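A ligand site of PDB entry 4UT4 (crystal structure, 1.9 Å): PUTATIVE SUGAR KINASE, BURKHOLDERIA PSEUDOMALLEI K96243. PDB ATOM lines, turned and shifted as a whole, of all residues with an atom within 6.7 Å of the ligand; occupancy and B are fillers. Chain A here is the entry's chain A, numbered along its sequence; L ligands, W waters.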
ATOM      1  N   ARG A  13     -29.610  25.254   8.935  1.00  0.00           N
ATOM      2  CA  ARG A  13     -29.272  26.186  10.000  1.00  0.00           C
ATOM      3  C   ARG A  13     -28.045  27.056   9.729  1.00  0.00           C
ATOM      4  O   ARG A  13     -27.089  26.667   9.045  1.00  0.00           O
ATOM      5  CB  ARG A  13     -29.104  25.419  11.327  1.00  0.00           C
ATOM      6  CG  ARG A  13     -27.917  24.443  11.341  1.00  0.00           C
ATOM      7  CD  ARG A  13     -26.666  25.040  12.014  1.00  0.00           C
ATOM      8  NE  ARG A  13     -25.481  24.195  11.822  1.00  0.00           N
ATOM      9  CZ  ARG A  13     -24.559  24.371  10.874  1.00  0.00           C
ATOM     10  NH1 ARG A  13     -24.658  25.384  10.023  1.00  0.00           N
ATOM     11  NH2 ARG A  13     -23.527  23.544  10.774  1.00  0.00           N
ATOM     12  N   GLY A  18     -19.938  29.636  18.166  1.00  0.00           N
ATOM     13  CA  GLY A  18     -19.582  28.473  18.992  1.00  0.00           C
ATOM     14  C   GLY A  18     -19.272  27.192  18.239  1.00  0.00           C
ATOM     15  O   GLY A  18     -18.745  26.246  18.834  1.00  0.00           O
ATOM     16  N   GLY A  19     -19.597  27.160  16.942  1.00  0.00           N
ATOM     17  CA  GLY A  19     -19.400  25.954  16.106  1.00  0.00           C
ATOM     18  C   GLY A  19     -17.964  25.454  16.186  1.00  0.00           C
ATOM     19  O   GLY A  19     -17.026  26.252  16.146  1.00  0.00           O
ATOM     20  N   GLY A  20     -17.797  24.151  16.327  1.00  0.00           N
ATOM     21  CA  GLY A  20     -16.477  23.577  16.606  1.00  0.00           C
ATOM     22  C   GLY A  20     -16.280  23.169  18.059  1.00  0.00           C
ATOM     23  O   GLY A  20     -15.621  22.159  18.336  1.00  0.00           O
ATOM     24  N   THR A  21     -16.825  23.943  19.001  1.00  0.00           N
ATOM     25  CA  THR A  21     -16.759  23.562  20.419  1.00  0.00           C
ATOM     26  C   THR A  21     -17.677  22.390  20.741  1.00  0.00           C
ATOM     27  O   THR A  21     -17.570  21.791  21.824  1.00  0.00           O
ATOM     28  CB  THR A  21     -17.012  24.738  21.404  1.00  0.00           C
ATOM     29  OG1 THR A  21     -18.400  25.127  21.385  1.00  0.00           O
ATOM     30  CG2 THR A  21     -16.132  25.954  21.093  1.00  0.00           C
ATOM     31  N   ASP A  22     -18.574  22.055  19.817  1.00  0.00           N
ATOM     32  CA  ASP A  22     -19.513  20.935  20.029  1.00  0.00           C
ATOM     33  C   ASP A  22     -18.942  19.587  19.600  1.00  0.00           C
ATOM     34  O   ASP A  22     -19.649  18.581  19.668  1.00  0.00           O
ATOM     35  CB  ASP A  22     -20.847  21.170  19.288  1.00  0.00           C
ATOM     36  CG  ASP A  22     -20.673  21.253  17.777  1.00  0.00           C
ATOM     37  OD1 ASP A  22     -19.738  21.929  17.319  1.00  0.00           O
ATOM     38  OD2 ASP A  22     -21.490  20.643  17.037  1.00  0.00           O
ATOM     39  N   VAL A  23     -17.689  19.575  19.125  1.00  0.00           N
ATOM     40  CA  VAL A  23     -17.077  18.335  18.649  1.00  0.00           C
ATOM     41  C   VAL A  23     -16.303  17.662  19.776  1.00  0.00           C
ATOM     42  O   VAL A  23     -15.655  18.332  20.572  1.00  0.00           O
ATOM     43  CB  VAL A  23     -16.201  18.541  17.392  1.00  0.00           C
ATOM     44  CG1 VAL A  23     -15.660  17.202  16.883  1.00  0.00           C
ATOM     45  CG2 VAL A  23     -17.015  19.215  16.296  1.00  0.00           C
ATOM     46  N   VAL A  34     -22.980  26.318  21.577  1.00  0.00           N
ATOM     47  CA  VAL A  34     -23.281  26.735  20.219  1.00  0.00           C
ATOM     48  C   VAL A  34     -24.552  27.556  20.211  1.00  0.00           C
ATOM     49  O   VAL A  34     -25.531  27.188  20.872  1.00  0.00           O
ATOM     50  CB  VAL A  34     -23.391  25.537  19.242  1.00  0.00           C
ATOM     51  CG1 VAL A  34     -23.996  25.972  17.909  1.00  0.00           C
ATOM     52  CG2 VAL A  34     -22.030  24.929  18.987  1.00  0.00           C
ATOM     53  N   GLY A 115     -22.223  24.632   4.441  1.00  0.00           N
ATOM     54  CA  GLY A 115     -22.077  25.269   5.752  1.00  0.00           C
ATOM     55  C   GLY A 115     -23.415  25.437   6.475  1.00  0.00           C
ATOM     56  O   GLY A 115     -23.499  26.136   7.476  1.00  0.00           O
ATOM     57  N   LEU A 116     -24.465  24.758   5.991  1.00  0.00           N
ATOM     58  CA  LEU A 116     -25.798  24.894   6.594  1.00  0.00           C
ATOM     59  C   LEU A 116     -26.258  23.668   7.366  1.00  0.00           C
ATOM     60  O   LEU A 116     -27.434  23.547   7.710  1.00  0.00           O
ATOM     61  CB  LEU A 116     -26.830  25.257   5.530  1.00  0.00           C
ATOM     62  CG  LEU A 116     -26.596  26.549   4.763  1.00  0.00           C
ATOM     63  CD1 LEU A 116     -27.692  26.667   3.713  1.00  0.00           C
ATOM     64  CD2 LEU A 116     -26.606  27.771   5.675  1.00  0.00           C
ATOM     65  N   GLY A 117     -25.330  22.753   7.651  1.00  0.00           N
ATOM     66  CA  GLY A 117     -25.677  21.574   8.435  1.00  0.00           C
ATOM     67  C   GLY A 117     -26.481  20.499   7.732  1.00  0.00           C
ATOM     68  O   GLY A 117     -27.159  19.707   8.386  1.00  0.00           O
ATOM     69  N   SER A 118     -26.402  20.437   6.405  1.00  0.00           N
ATOM     70  CA  SER A 118     -27.320  19.547   5.657  1.00  0.00           C
ATOM     71  C   SER A 118     -27.067  18.057   5.874  1.00  0.00           C
ATOM     72  O   SER A 118     -28.021  17.259   5.899  1.00  0.00           O
ATOM     73  CB  SER A 118     -27.301  19.872   4.162  1.00  0.00           C
ATOM     74  OG  SER A 118     -26.124  19.403   3.536  1.00  0.00           O
ATOM     75  N   SER A 120     -26.306  16.276   8.594  1.00  0.00           N
ATOM     76  CA  SER A 120     -27.049  15.783   9.770  1.00  0.00           C
ATOM     77  C   SER A 120     -28.535  16.087   9.655  1.00  0.00           C
ATOM     78  O   SER A 120     -29.379  15.336  10.135  1.00  0.00           O
ATOM     79  CB  SER A 120     -26.502  16.403  11.050  1.00  0.00           C
ATOM     80  OG  SER A 120     -25.124  16.110  11.231  1.00  0.00           O
ATOM     81  N   GLU A 151     -25.322   8.578  12.486  1.00  0.00           N
ATOM     82  CA  GLU A 151     -24.329   9.176  11.613  1.00  0.00           C
ATOM     83  C   GLU A 151     -22.898   8.991  12.122  1.00  0.00           C
ATOM     84  O   GLU A 151     -21.999   8.625  11.348  1.00  0.00           O
ATOM     85  CB  GLU A 151     -24.649  10.670  11.390  1.00  0.00           C
ATOM     86  CG  GLU A 151     -23.592  11.393  10.546  1.00  0.00           C
ATOM     87  CD  GLU A 151     -23.845  12.866  10.368  1.00  0.00           C
ATOM     88  OE1 GLU A 151     -24.799  13.391  10.970  1.00  0.00           O
ATOM     89  OE2 GLU A 151     -23.080  13.513   9.631  1.00  0.00           O
ATOM     90  N   ARG A 152     -22.713   9.200  13.417  1.00  0.00           N
ATOM     91  CA  ARG A 152     -21.378   9.281  13.998  1.00  0.00           C
ATOM     92  C   ARG A 152     -20.862   7.919  14.451  1.00  0.00           C
ATOM     93  O   ARG A 152     -19.660   7.684  14.396  1.00  0.00           O
ATOM     94  CB  ARG A 152     -21.358  10.248  15.170  1.00  0.00           C
ATOM     95  CG  ARG A 152     -21.888  11.638  14.828  1.00  0.00           C
ATOM     96  CD  ARG A 152     -20.779  12.669  14.709  1.00  0.00           C
ATOM     97  NE  ARG A 152     -21.384  13.982  14.427  1.00  0.00           N
ATOM     98  CZ  ARG A 152     -21.656  14.434  13.207  1.00  0.00           C
ATOM     99  NH1 ARG A 152     -21.325  13.718  12.144  1.00  0.00           N
ATOM    100  NH2 ARG A 152     -22.214  15.625  13.066  1.00  0.00           N
ATOM    101  N   ALA A 158     -17.336  11.571  11.413  1.00  0.00           N
ATOM    102  CA  ALA A 158     -16.927  12.447  12.525  1.00  0.00           C
ATOM    103  C   ALA A 158     -17.638  13.792  12.448  1.00  0.00           C
ATOM    104  O   ALA A 158     -17.971  14.256  11.363  1.00  0.00           O
ATOM    105  CB  ALA A 158     -15.418  12.658  12.531  1.00  0.00           C
ATOM    106  N   GLY A 159     -17.871  14.401  13.603  1.00  0.00           N
ATOM    107  CA  GLY A 159     -18.468  15.737  13.614  1.00  0.00           C
ATOM    108  C   GLY A 159     -19.046  16.055  14.972  1.00  0.00           C
ATOM    109  O   GLY A 159     -18.790  15.338  15.937  1.00  0.00           O
ATOM    110  N   GLY A 160     -19.836  17.122  15.056  1.00  0.00           N
ATOM    111  CA  GLY A 160     -20.395  17.553  16.345  1.00  0.00           C
ATOM    112  C   GLY A 160     -21.842  17.168  16.542  1.00  0.00           C
ATOM    113  O   GLY A 160     -22.339  16.199  15.951  1.00  0.00           O
ATOM    114  N   ARG A 161     -22.530  17.961  17.369  1.00  0.00           N
ATOM    115  CA  ARG A 161     -23.866  17.641  17.807  1.00  0.00           C
ATOM    116  C   ARG A 161     -24.894  18.721  17.460  1.00  0.00           C
ATOM    117  O   ARG A 161     -26.100  18.493  17.591  1.00  0.00           O
ATOM    118  CB  ARG A 161     -23.861  17.453  19.336  1.00  0.00           C
ATOM    119  CG  ARG A 161     -23.828  16.006  19.831  1.00  0.00           C
ATOM    120  CD  ARG A 161     -23.839  15.961  21.359  1.00  0.00           C
ATOM    121  NE  ARG A 161     -22.499  16.165  21.914  1.00  0.00           N
ATOM    122  CZ  ARG A 161     -22.234  16.344  23.211  1.00  0.00           C
ATOM    123  NH1 ARG A 161     -23.220  16.395  24.107  1.00  0.00           N
ATOM    124  NH2 ARG A 161     -20.979  16.481  23.616  1.00  0.00           N
ATOM    125  N   GLN A 162     -24.442  19.894  17.041  1.00  0.00           N
ATOM    126  CA  GLN A 162     -25.362  21.042  16.960  1.00  0.00           C
ATOM    127  C   GLN A 162     -26.409  20.878  15.862  1.00  0.00           C
ATOM    128  O   GLN A 162     -27.520  21.373  16.009  1.00  0.00           O
ATOM    129  CB  GLN A 162     -24.611  22.372  16.758  1.00  0.00           C
ATOM    130  CG  GLN A 162     -23.812  22.440  15.460  1.00  0.00           C
ATOM    131  CD  GLN A 162     -23.638  23.860  14.907  1.00  0.00           C
ATOM    132  OE1 GLN A 162     -24.587  24.639  14.834  1.00  0.00           O
ATOM    133  NE2 GLN A 162     -22.412  24.186  14.464  1.00  0.00           N
ATOM    134  N   ASP A 163     -26.059  20.219  14.754  1.00  0.00           N
ATOM    135  CA  ASP A 163     -26.961  20.143  13.593  1.00  0.00           C
ATOM    136  C   ASP A 163     -28.151  19.252  13.855  1.00  0.00           C
ATOM    137  O   ASP A 163     -29.254  19.516  13.340  1.00  0.00           O
ATOM    138  CB  ASP A 163     -26.230  19.617  12.356  1.00  0.00           C
ATOM    139  CG  ASP A 163     -24.998  20.439  12.004  1.00  0.00           C
ATOM    140  OD1 ASP A 163     -24.827  21.558  12.542  1.00  0.00           O
ATOM    141  OD2 ASP A 163     -24.212  19.951  11.157  1.00  0.00           O
ATOM    142  N   GLN A 164     -27.933  18.181  14.605  1.00  0.00           N
ATOM    143  CA  GLN A 164     -29.016  17.242  14.947  1.00  0.00           C
ATOM    144  C   GLN A 164     -30.099  17.958  15.720  1.00  0.00           C
ATOM    145  O   GLN A 164     -31.283  17.718  15.533  1.00  0.00           O
ATOM    146  CB  GLN A 164     -28.493  16.064  15.774  1.00  0.00           C
ATOM    147  CG  GLN A 164     -27.674  15.042  15.005  1.00  0.00           C
ATOM    148  CD  GLN A 164     -26.230  15.434  14.765  1.00  0.00           C
ATOM    149  OE1 GLN A 164     -25.738  16.443  15.289  1.00  0.00           O
ATOM    150  NE2 GLN A 164     -25.533  14.635  13.974  1.00  0.00           N
ATOM    151  N   SER A 213     -14.514  20.877   5.690  1.00  0.00           N
ATOM    152  CA  SER A 213     -15.132  20.536   6.966  1.00  0.00           C
ATOM    153  C   SER A 213     -14.419  19.427   7.714  1.00  0.00           C
ATOM    154  O   SER A 213     -14.152  19.559   8.901  1.00  0.00           O
ATOM    155  CB  SER A 213     -16.613  20.145   6.793  1.00  0.00           C
ATOM    156  OG  SER A 213     -17.395  21.286   6.525  1.00  0.00           O
ATOM    157  N   ILE A 216     -10.971  20.639   8.971  1.00  0.00           N
ATOM    158  CA  ILE A 216     -11.061  21.612  10.086  1.00  0.00           C
ATOM    159  C   ILE A 216     -11.394  20.911  11.411  1.00  0.00           C
ATOM    160  O   ILE A 216     -10.806  21.204  12.457  1.00  0.00           O
ATOM    161  CB  ILE A 216     -12.079  22.746   9.792  1.00  0.00           C
ATOM    162  CG1 ILE A 216     -11.554  23.620   8.629  1.00  0.00           C
ATOM    163  CG2 ILE A 216     -12.363  23.552  11.068  1.00  0.00           C
ATOM    164  CD1 ILE A 216     -12.612  24.393   7.835  1.00  0.00           C
ATOM    165  N   ILE A 217     -12.328  19.972  11.347  1.00  0.00           N
ATOM    166  CA  ILE A 217     -12.787  19.266  12.518  1.00  0.00           C
ATOM    167  C   ILE A 217     -11.657  18.357  13.026  1.00  0.00           C
ATOM    168  O   ILE A 217     -11.419  18.263  14.234  1.00  0.00           O
ATOM    169  CB  ILE A 217     -14.100  18.512  12.194  1.00  0.00           C
ATOM    170  CG1 ILE A 217     -15.284  19.471  12.357  1.00  0.00           C
ATOM    171  CG2 ILE A 217     -14.286  17.268  13.050  1.00  0.00           C
ATOM    172  CD1 ILE A 217     -16.439  19.177  11.419  1.00  0.00           C
ATOM    173  N   GLN A 220      -9.149  20.730  14.712  1.00  0.00           N
ATOM    174  CA  GLN A 220      -9.636  21.203  16.003  1.00  0.00           C
ATOM    175  C   GLN A 220      -9.569  20.094  17.060  1.00  0.00           C
ATOM    176  O   GLN A 220      -9.295  20.353  18.237  1.00  0.00           O
ATOM    177  CB  GLN A 220     -11.051  21.769  15.882  1.00  0.00           C
ATOM    178  CG  GLN A 220     -11.057  23.095  15.130  1.00  0.00           C
ATOM    179  CD  GLN A 220     -12.449  23.577  14.751  1.00  0.00           C
ATOM    180  OE1 GLN A 220     -13.385  22.787  14.603  1.00  0.00           O
ATOM    181  NE2 GLN A 220     -12.581  24.883  14.572  1.00  0.00           N
ATOM    182  N   LYS A 268     -12.243  31.801  15.512  1.00  0.00           N
ATOM    183  CA  LYS A 268     -12.541  30.667  14.654  1.00  0.00           C
ATOM    184  C   LYS A 268     -11.417  30.463  13.625  1.00  0.00           C
ATOM    185  O   LYS A 268     -10.943  29.333  13.440  1.00  0.00           O
ATOM    186  CB  LYS A 268     -13.909  30.899  13.950  1.00  0.00           C
ATOM    187  CG  LYS A 268     -14.463  29.673  13.230  1.00  0.00           C
ATOM    188  CD  LYS A 268     -15.687  30.109  12.404  1.00  0.00           C
ATOM    189  CE  LYS A 268     -16.259  28.956  11.607  1.00  0.00           C
ATOM    190  NZ  LYS A 268     -16.886  27.911  12.447  1.00  0.00           N
ATOM    191  N   GLY A 299     -20.984  27.163   9.494  1.00  0.00           N
ATOM    192  CA  GLY A 299     -20.350  25.855   9.410  1.00  0.00           C
ATOM    193  C   GLY A 299     -18.853  25.917   9.730  1.00  0.00           C
ATOM    194  O   GLY A 299     -18.359  26.910  10.239  1.00  0.00           O
ATOM    195  N   ALA A 300     -18.142  24.833   9.425  1.00  0.00           N
ATOM    196  CA  ALA A 300     -16.757  24.664   9.879  1.00  0.00           C
ATOM    197  C   ALA A 300     -15.839  25.712   9.277  1.00  0.00           C
ATOM    198  O   ALA A 300     -14.950  26.244   9.954  1.00  0.00           O
ATOM    199  CB  ALA A 300     -16.259  23.248   9.568  1.00  0.00           C
ATOM    200  N   GLY A 301     -16.085  26.053   8.003  1.00  0.00           N
ATOM    201  CA  GLY A 301     -15.237  27.019   7.329  1.00  0.00           C
ATOM    202  C   GLY A 301     -14.789  26.519   5.973  1.00  0.00           C
ATOM    203  O   GLY A 301     -15.218  25.443   5.529  1.00  0.00           O
HETATM  204  C1  LIG L   1     -20.862  20.163  11.059  1.00  0.00           C
HETATM  205  C2  LIG L   1     -21.232  19.328  12.299  1.00  0.00           C
HETATM  206  C3  LIG L   1     -21.425  20.238  13.517  1.00  0.00           C
HETATM  207  C4  LIG L   1     -20.242  21.198  13.728  1.00  0.00           C
HETATM  208  C5  LIG L   1     -19.882  21.908  12.414  1.00  0.00           C
HETATM  209  C6  LIG L   1     -18.630  22.759  12.555  1.00  0.00           C
HETATM  210  O1  LIG L   1     -21.992  20.925  10.658  1.00  0.00           O
HETATM  211  O2  LIG L   1     -20.236  18.336  12.544  1.00  0.00           O
HETATM  212  O3  LIG L   1     -21.701  19.439  14.642  1.00  0.00           O
HETATM  213  O4  LIG L   1     -20.528  22.178  14.692  1.00  0.00           O
HETATM  214  O5  LIG L   1     -19.744  21.011  11.323  1.00  0.00           O
HETATM  215  O6  LIG L   1     -17.504  21.938  12.771  1.00  0.00           O
HETATM  216  O   HOH W   1     -19.709  16.605  10.541  1.00  0.00           O
HETATM  217  O   HOH W   2     -23.916  18.195  14.080  1.00  0.00           O
HETATM  218  O   HOH W   3     -22.282  19.560   7.921  1.00  0.00           O
HETATM  219  O   HOH W   4     -19.316  22.319   8.664  1.00  0.00           O
HETATM  220  O   HOH W   5     -15.579  23.459  13.326  1.00  0.00           O
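An oxygen (O2) of the ligand lies within hydrogen-bond range of the guanidinium group (NH2) of Arg 152, 3.4 Å away. The side-chain amide nitrogen of Gln 162 is in hydrogen-bond range of an oxygen (O4) of the ligand. The guanidinium group (NH2) of Arg 13 is in hydrogen-bond range of an oxygen (O1) of the ligand (3.0 Å). The backbone NH (N) of Arg 161 sits at hydrogen-bond distance from an oxygen (O3) of the ligand (3.2 Å). An oxygen (O2) of the ligand is in hydrogen-bond range of the backbone NH of Gly 160. O1 of the ligand sits at hydrogen-bond distance from OD2 of Asp 163, at 2.5 Å. An oxygen (O3) of the ligand is in hydrogen-bond range of the side-chain carboxylate of Asp 22, 2.7 Å away.
The side-chain amide oxygen (OE1) of Gln 162 is in hydrogen-bond range of the guanidinium group (NE) of Arg 13, 3.2 Å away. The backbone carbonyl oxygen of Leu 116 lies within hydrogen-bond range of the backbone NH of Arg 13, at 3.0 Å. The backbone carbonyl oxygen (O) of Gly 159 lies close to the guanidinium group (NE) of Arg 152 (3.3 Å). The side-chain carboxylate of Asp 22 sits at hydrogen-bond distance from the backbone NH of Gly 20 (3.1 Å). The backbone carbonyl oxygen (O) of Arg 161 sits close to the side-chain amide oxygen (OE1) of Gln 164, at 3.1 Å. The side-chain carboxylate of Asp 22 lies within hydrogen-bond range of the backbone NH of Gln 162 (3.0 Å). N of Arg 161 sits at hydrogen-bond distance from OD2 of Asp 22 (2.9 Å). NH1 of Arg 152 is in salt-bridge range of OE2 of Glu 151 (3.1 Å).
Merely in contact with the ligand: Gly 20, Gly 159, Ile 217 and Ala 300.
Water W5 bridges an oxygen (O6) of the ligand (2.5 Å) and the side-chain amide oxygen (OE1) of Gln 220 (2.6 Å). Water W1 bridges O2 of the ligand (2.7 Å) and O of Ala 158 (3.0 Å). Water W4 lies within hydrogen-bond range of N of Ala 300, O5 of the ligand and OG of Ser 213.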
